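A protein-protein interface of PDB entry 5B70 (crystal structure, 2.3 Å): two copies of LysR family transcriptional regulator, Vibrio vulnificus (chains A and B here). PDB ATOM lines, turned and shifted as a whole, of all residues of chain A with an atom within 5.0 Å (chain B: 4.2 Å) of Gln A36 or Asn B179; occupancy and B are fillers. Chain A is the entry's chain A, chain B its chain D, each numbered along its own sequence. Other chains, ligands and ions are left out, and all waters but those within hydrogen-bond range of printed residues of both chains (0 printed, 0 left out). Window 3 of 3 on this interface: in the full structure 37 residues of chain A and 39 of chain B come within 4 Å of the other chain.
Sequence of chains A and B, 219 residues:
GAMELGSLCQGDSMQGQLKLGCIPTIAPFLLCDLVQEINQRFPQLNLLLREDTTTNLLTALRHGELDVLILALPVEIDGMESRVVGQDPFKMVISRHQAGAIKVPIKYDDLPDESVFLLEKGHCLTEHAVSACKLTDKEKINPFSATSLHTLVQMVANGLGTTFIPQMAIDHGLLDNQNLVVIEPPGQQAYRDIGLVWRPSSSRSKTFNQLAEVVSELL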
ATOM      1  N   CYS A  32       6.057  18.289  31.048  1.00  0.00           N
ATOM      2  CA  CYS A  32       6.041  17.174  30.105  1.00  0.00           C
ATOM      3  C   CYS A  32       4.619  16.702  29.841  1.00  0.00           C
ATOM      4  O   CYS A  32       4.251  16.424  28.694  1.00  0.00           O
ATOM      5  CB  CYS A  32       6.893  16.022  30.629  1.00  0.00           C
ATOM      6  SG  CYS A  32       8.617  16.452  30.902  1.00  0.00           S
ATOM      7  N   ASP A  33       3.805  16.612  30.894  1.00  0.00           N
ATOM      8  CA  ASP A  33       2.418  16.195  30.732  1.00  0.00           C
ATOM      9  C   ASP A  33       1.563  17.315  30.156  1.00  0.00           C
ATOM     10  O   ASP A  33       0.664  17.059  29.347  1.00  0.00           O
ATOM     11  CB  ASP A  33       1.852  15.738  32.075  1.00  0.00           C
ATOM     12  CG  ASP A  33       2.752  14.742  32.772  1.00  0.00           C
ATOM     13  OD1 ASP A  33       3.012  14.923  33.981  1.00  0.00           O
ATOM     14  OD2 ASP A  33       3.197  13.781  32.110  1.00  0.00           O
ATOM     15  N   LEU A  34       1.831  18.559  30.561  1.00  0.00           N
ATOM     16  CA  LEU A  34       1.030  19.683  30.088  1.00  0.00           C
ATOM     17  C   LEU A  34       1.109  19.823  28.571  1.00  0.00           C
ATOM     18  O   LEU A  34       0.102  20.115  27.914  1.00  0.00           O
ATOM     19  CB  LEU A  34       1.483  20.969  30.775  1.00  0.00           C
ATOM     20  CG  LEU A  34       0.660  22.216  30.461  1.00  0.00           C
ATOM     21  CD1 LEU A  34      -0.757  22.039  30.966  1.00  0.00           C
ATOM     22  CD2 LEU A  34       1.303  23.460  31.069  1.00  0.00           C
ATOM     23  N   VAL A  35       2.293  19.606  27.992  1.00  0.00           N
ATOM     24  CA  VAL A  35       2.442  19.729  26.544  1.00  0.00           C
ATOM     25  C   VAL A  35       1.660  18.634  25.831  1.00  0.00           C
ATOM     26  O   VAL A  35       0.934  18.897  24.864  1.00  0.00           O
ATOM     27  CB  VAL A  35       3.930  19.708  26.150  1.00  0.00           C
ATOM     28  CG1 VAL A  35       4.079  19.431  24.663  1.00  0.00           C
ATOM     29  CG2 VAL A  35       4.585  21.030  26.506  1.00  0.00           C
ATOM     30  N   GLN A  36       1.798  17.388  26.293  1.00  0.00           N
ATOM     31  CA  GLN A  36       1.075  16.290  25.661  1.00  0.00           C
ATOM     32  C   GLN A  36      -0.432  16.457  25.805  1.00  0.00           C
ATOM     33  O   GLN A  36      -1.190  16.012  24.936  1.00  0.00           O
ATOM     34  CB  GLN A  36       1.525  14.954  26.251  1.00  0.00           C
ATOM     35  CG  GLN A  36       3.012  14.695  26.125  1.00  0.00           C
ATOM     36  CD  GLN A  36       3.486  14.713  24.686  1.00  0.00           C
ATOM     37  OE1 GLN A  36       2.868  14.109  23.810  1.00  0.00           O
ATOM     38  NE2 GLN A  36       4.587  15.415  24.434  1.00  0.00           N
ATOM     39  N   GLU A  37      -0.885  17.096  26.888  1.00  0.00           N
ATOM     40  CA  GLU A  37      -2.311  17.371  27.032  1.00  0.00           C
ATOM     41  C   GLU A  37      -2.768  18.419  26.025  1.00  0.00           C
ATOM     42  O   GLU A  37      -3.755  18.216  25.309  1.00  0.00           O
ATOM     43  CB  GLU A  37      -2.625  17.821  28.461  1.00  0.00           C
ATOM     44  CG  GLU A  37      -2.556  16.707  29.499  1.00  0.00           C
ATOM     45  CD  GLU A  37      -3.659  15.675  29.330  1.00  0.00           C
ATOM     46  OE1 GLU A  37      -4.769  16.047  28.893  1.00  0.00           O
ATOM     47  OE2 GLU A  37      -3.414  14.485  29.627  1.00  0.00           O
ATOM     48  N   ILE A  38      -2.044  19.540  25.944  1.00  0.00           N
ATOM     49  CA  ILE A  38      -2.444  20.641  25.072  1.00  0.00           C
ATOM     50  C   ILE A  38      -2.424  20.223  23.606  1.00  0.00           C
ATOM     51  O   ILE A  38      -3.276  20.654  22.819  1.00  0.00           O
ATOM     52  CB  ILE A  38      -1.545  21.869  25.336  1.00  0.00           C
ATOM     53  CG1 ILE A  38      -2.204  22.814  26.346  1.00  0.00           C
ATOM     54  CG2 ILE A  38      -1.220  22.612  24.047  1.00  0.00           C
ATOM     55  CD1 ILE A  38      -2.423  22.208  27.712  1.00  0.00           C
ATOM     56  N   ASN A  39      -1.479  19.358  23.219  1.00  0.00           N
ATOM     57  CA  ASN A  39      -1.382  18.940  21.822  1.00  0.00           C
ATOM     58  C   ASN A  39      -2.661  18.272  21.333  1.00  0.00           C
ATOM     59  O   ASN A  39      -2.993  18.366  20.144  1.00  0.00           O
ATOM     60  CB  ASN A  39      -0.193  17.997  21.631  1.00  0.00           C
ATOM     61  CG  ASN A  39       1.139  18.710  21.727  1.00  0.00           C
ATOM     62  OD1 ASN A  39       1.232  19.914  21.482  1.00  0.00           O
ATOM     63  ND2 ASN A  39       2.183  17.969  22.081  1.00  0.00           N
ATOM     64  N   GLN A  40      -3.390  17.599  22.222  1.00  0.00           N
ATOM     65  CA  GLN A  40      -4.650  16.950  21.877  1.00  0.00           C
ATOM     66  C   GLN A  40      -5.870  17.797  22.217  1.00  0.00           C
ATOM     67  O   GLN A  40      -6.795  17.891  21.404  1.00  0.00           O
ATOM     68  CB  GLN A  40      -4.768  15.598  22.587  1.00  0.00           C
ATOM     69  CG  GLN A  40      -6.088  14.889  22.323  1.00  0.00           C
ATOM     70  CD  GLN A  40      -6.574  14.088  23.515  1.00  0.00           C
ATOM     71  OE1 GLN A  40      -7.523  14.478  24.192  1.00  0.00           O
ATOM     72  NE2 GLN A  40      -5.928  12.960  23.773  1.00  0.00           N
ATOM     73  N   SER B  95       8.293  15.886  17.014  1.00  0.00           N
ATOM     74  CA  SER B  95       7.091  15.188  17.440  1.00  0.00           C
ATOM     75  C   SER B  95       6.513  14.385  16.277  1.00  0.00           C
ATOM     76  O   SER B  95       6.903  14.546  15.118  1.00  0.00           O
ATOM     77  CB  SER B  95       6.051  16.170  17.979  1.00  0.00           C
ATOM     78  OG  SER B  95       5.576  17.019  16.952  1.00  0.00           O
ATOM     79  N   ARG B  96       5.567  13.505  16.596  1.00  0.00           N
ATOM     80  CA  ARG B  96       4.940  12.693  15.563  1.00  0.00           C
ATOM     81  C   ARG B  96       3.790  13.402  14.859  1.00  0.00           C
ATOM     82  O   ARG B  96       3.208  12.828  13.933  1.00  0.00           O
ATOM     83  CB  ARG B  96       4.459  11.367  16.151  1.00  0.00           C
ATOM     84  CG  ARG B  96       5.545  10.314  16.181  1.00  0.00           C
ATOM     85  CD  ARG B  96       4.969   8.925  16.319  1.00  0.00           C
ATOM     86  NE  ARG B  96       5.926   7.908  15.899  1.00  0.00           N
ATOM     87  CZ  ARG B  96       6.871   7.402  16.684  1.00  0.00           C
ATOM     88  NH1 ARG B  96       6.988   7.821  17.939  1.00  0.00           N
ATOM     89  NH2 ARG B  96       7.699   6.477  16.214  1.00  0.00           N
ATOM     90  N   HIS B  97       3.449  14.629  15.266  1.00  0.00           N
ATOM     91  CA  HIS B  97       2.515  15.428  14.480  1.00  0.00           C
ATOM     92  C   HIS B  97       3.181  15.957  13.216  1.00  0.00           C
ATOM     93  O   HIS B  97       2.562  15.989  12.146  1.00  0.00           O
ATOM     94  CB  HIS B  97       1.973  16.590  15.311  1.00  0.00           C
ATOM     95  CG  HIS B  97       1.879  16.299  16.774  1.00  0.00           C
ATOM     96  ND1 HIS B  97       1.272  15.166  17.271  1.00  0.00           N
ATOM     97  CD2 HIS B  97       2.312  16.997  17.850  1.00  0.00           C
ATOM     98  CE1 HIS B  97       1.338  15.177  18.591  1.00  0.00           C
ATOM     99  NE2 HIS B  97       1.964  16.277  18.967  1.00  0.00           N
ATOM    100  N   ALA B 157       8.367  18.841  21.643  1.00  0.00           N
ATOM    101  CA  ALA B 157       7.264  17.908  21.849  1.00  0.00           C
ATOM    102  C   ALA B 157       5.923  18.537  21.496  1.00  0.00           C
ATOM    103  O   ALA B 157       4.995  17.833  21.079  1.00  0.00           O
ATOM    104  CB  ALA B 157       7.252  17.417  23.297  1.00  0.00           C
ATOM    105  N   ASN B 177       7.837   9.529  26.946  1.00  0.00           N
ATOM    106  CA  ASN B 177       6.426   9.912  27.031  1.00  0.00           C
ATOM    107  C   ASN B 177       6.171  11.316  26.499  1.00  0.00           C
ATOM    108  O   ASN B 177       5.200  11.972  26.888  1.00  0.00           O
ATOM    109  CB  ASN B 177       5.888   9.774  28.460  1.00  0.00           C
ATOM    110  CG  ASN B 177       5.979   8.354  28.980  1.00  0.00           C
ATOM    111  OD1 ASN B 177       5.163   7.505  28.622  1.00  0.00           O
ATOM    112  ND2 ASN B 177       6.951   8.095  29.848  1.00  0.00           N
ATOM    113  N   GLN B 178       7.027  11.788  25.597  1.00  0.00           N
ATOM    114  CA  GLN B 178       6.820  13.075  24.950  1.00  0.00           C
ATOM    115  C   GLN B 178       6.516  12.933  23.465  1.00  0.00           C
ATOM    116  O   GLN B 178       6.417  13.946  22.764  1.00  0.00           O
ATOM    117  CB  GLN B 178       8.025  13.984  25.186  1.00  0.00           C
ATOM    118  CG  GLN B 178       7.898  14.767  26.486  1.00  0.00           C
ATOM    119  CD  GLN B 178       9.192  15.401  26.929  1.00  0.00           C
ATOM    120  OE1 GLN B 178      10.258  14.790  26.848  1.00  0.00           O
ATOM    121  NE2 GLN B 178       9.109  16.631  27.413  1.00  0.00           N
ATOM    122  N   ASN B 179       6.375  11.703  22.969  1.00  0.00           N
ATOM    123  CA  ASN B 179       5.893  11.437  21.612  1.00  0.00           C
ATOM    124  C   ASN B 179       6.816  12.060  20.564  1.00  0.00           C
ATOM    125  O   ASN B 179       6.414  12.896  19.753  1.00  0.00           O
ATOM    126  CB  ASN B 179       4.452  11.935  21.450  1.00  0.00           C
ATOM    127  CG  ASN B 179       3.715  11.225  20.338  1.00  0.00           C
ATOM    128  OD1 ASN B 179       4.038  10.088  19.993  1.00  0.00           O
ATOM    129  ND2 ASN B 179       2.715  11.889  19.773  1.00  0.00           N
ATOM    130  N   LEU B 180       8.073  11.628  20.590  1.00  0.00           N
ATOM    131  CA  LEU B 180       9.100  12.170  19.719  1.00  0.00           C
ATOM    132  C   LEU B 180       9.700  11.071  18.856  1.00  0.00           C
ATOM    133  O   LEU B 180       9.534   9.877  19.121  1.00  0.00           O
ATOM    134  CB  LEU B 180      10.202  12.850  20.533  1.00  0.00           C
ATOM    135  CG  LEU B 180       9.718  13.981  21.436  1.00  0.00           C
ATOM    136  CD1 LEU B 180      10.865  14.504  22.275  1.00  0.00           C
ATOM    137  CD2 LEU B 180       9.113  15.087  20.595  1.00  0.00           C
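The side-chain amide nitrogen (NE2) of Gln B178 sits at hydrogen-bond distance from the side-chain sulfur (SG) of Cys A32, 3.5 Å away.
O of Gln B178 is in hydrogen-bond range of NE2 of Gln A36 (2.9 Å).
The side-chain amide nitrogen of Asn A39 lies within hydrogen-bond range of the backbone carbonyl oxygen of Ala B157 (3.0 Å).
No position is printed for both chains.
Of the 8 pairs that touch across the chains among the printed residues, none has its exchanged pair printed and touching as well.
Printed residues of chain B within 4 Å of Cys A32: Gln B178.
Of the printed residues of chain B, Val A35 touches Ala B157 (3.8 Å).
Of the printed residues of chain B, Gln A36 touches Ala B157, Asn B177, Gln B178 and Asn B179.
Gln A40 touches none of the printed residues of chain B.
Ser B95 touches none of the printed residues of chain A.
Of the printed residues of chain A, His B97 touches Asn A39 (3.6 Å).
Printed residues of chain A within 4 Å of Asn B177: Gln A36 (3.6 Å).
Printed residues of chain A within 4 Å of Asn B179: Gln A36 (3.6 Å).
The nearest printed residue of chain A that does not touch Asn B179 is Asn A39 (6.5 Å).
The backbone carbonyl oxygen (O) of Val A35 sits close to the side-chain amide nitrogen (ND2) of Asn A39, 3.2 Å away.
The backbone NH (N) of Arg B96 sits at hydrogen-bond distance from the backbone carbonyl oxygen (O) of Asn B179 (3.3 Å).
Of the 8 printed residues of chain B, 5 touch a printed residue of chain A.
Hydrophobic or aromatic side chains of chain B within 4 Å of the printed part of chain A: His B97 and Ala B157.
Of the 9 printed residues of chain A, 4 touch a printed residue of chain B.
Printed residues of chain A that touch a printed residue of chain B: Cys A32, Val A35, Gln A36 and Asn A39.
Hydrophobic or aromatic side chains of chain A within 4 Å of the printed part of chain B: Val A35.
Along chain A the printed residues that touch a printed residue of chain B span positions 32 to 39.
Among the printed residues, no Asp or Glu carboxylate lies within 4 Å of a Lys or Arg side-chain nitrogen of the other chain.
Ala B157 touches Val A35 (C to CG1, 3.8 Å).
CB of Ala B157 touches NE2 of Gln A36, 3.5 Å away.
CG of Gln A36 touches O of Asn B177, at 3.6 Å.
Gln A36 touches Asn B179 (OE1 to CB, 3.6 Å).
Asn A39 touches His B97.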
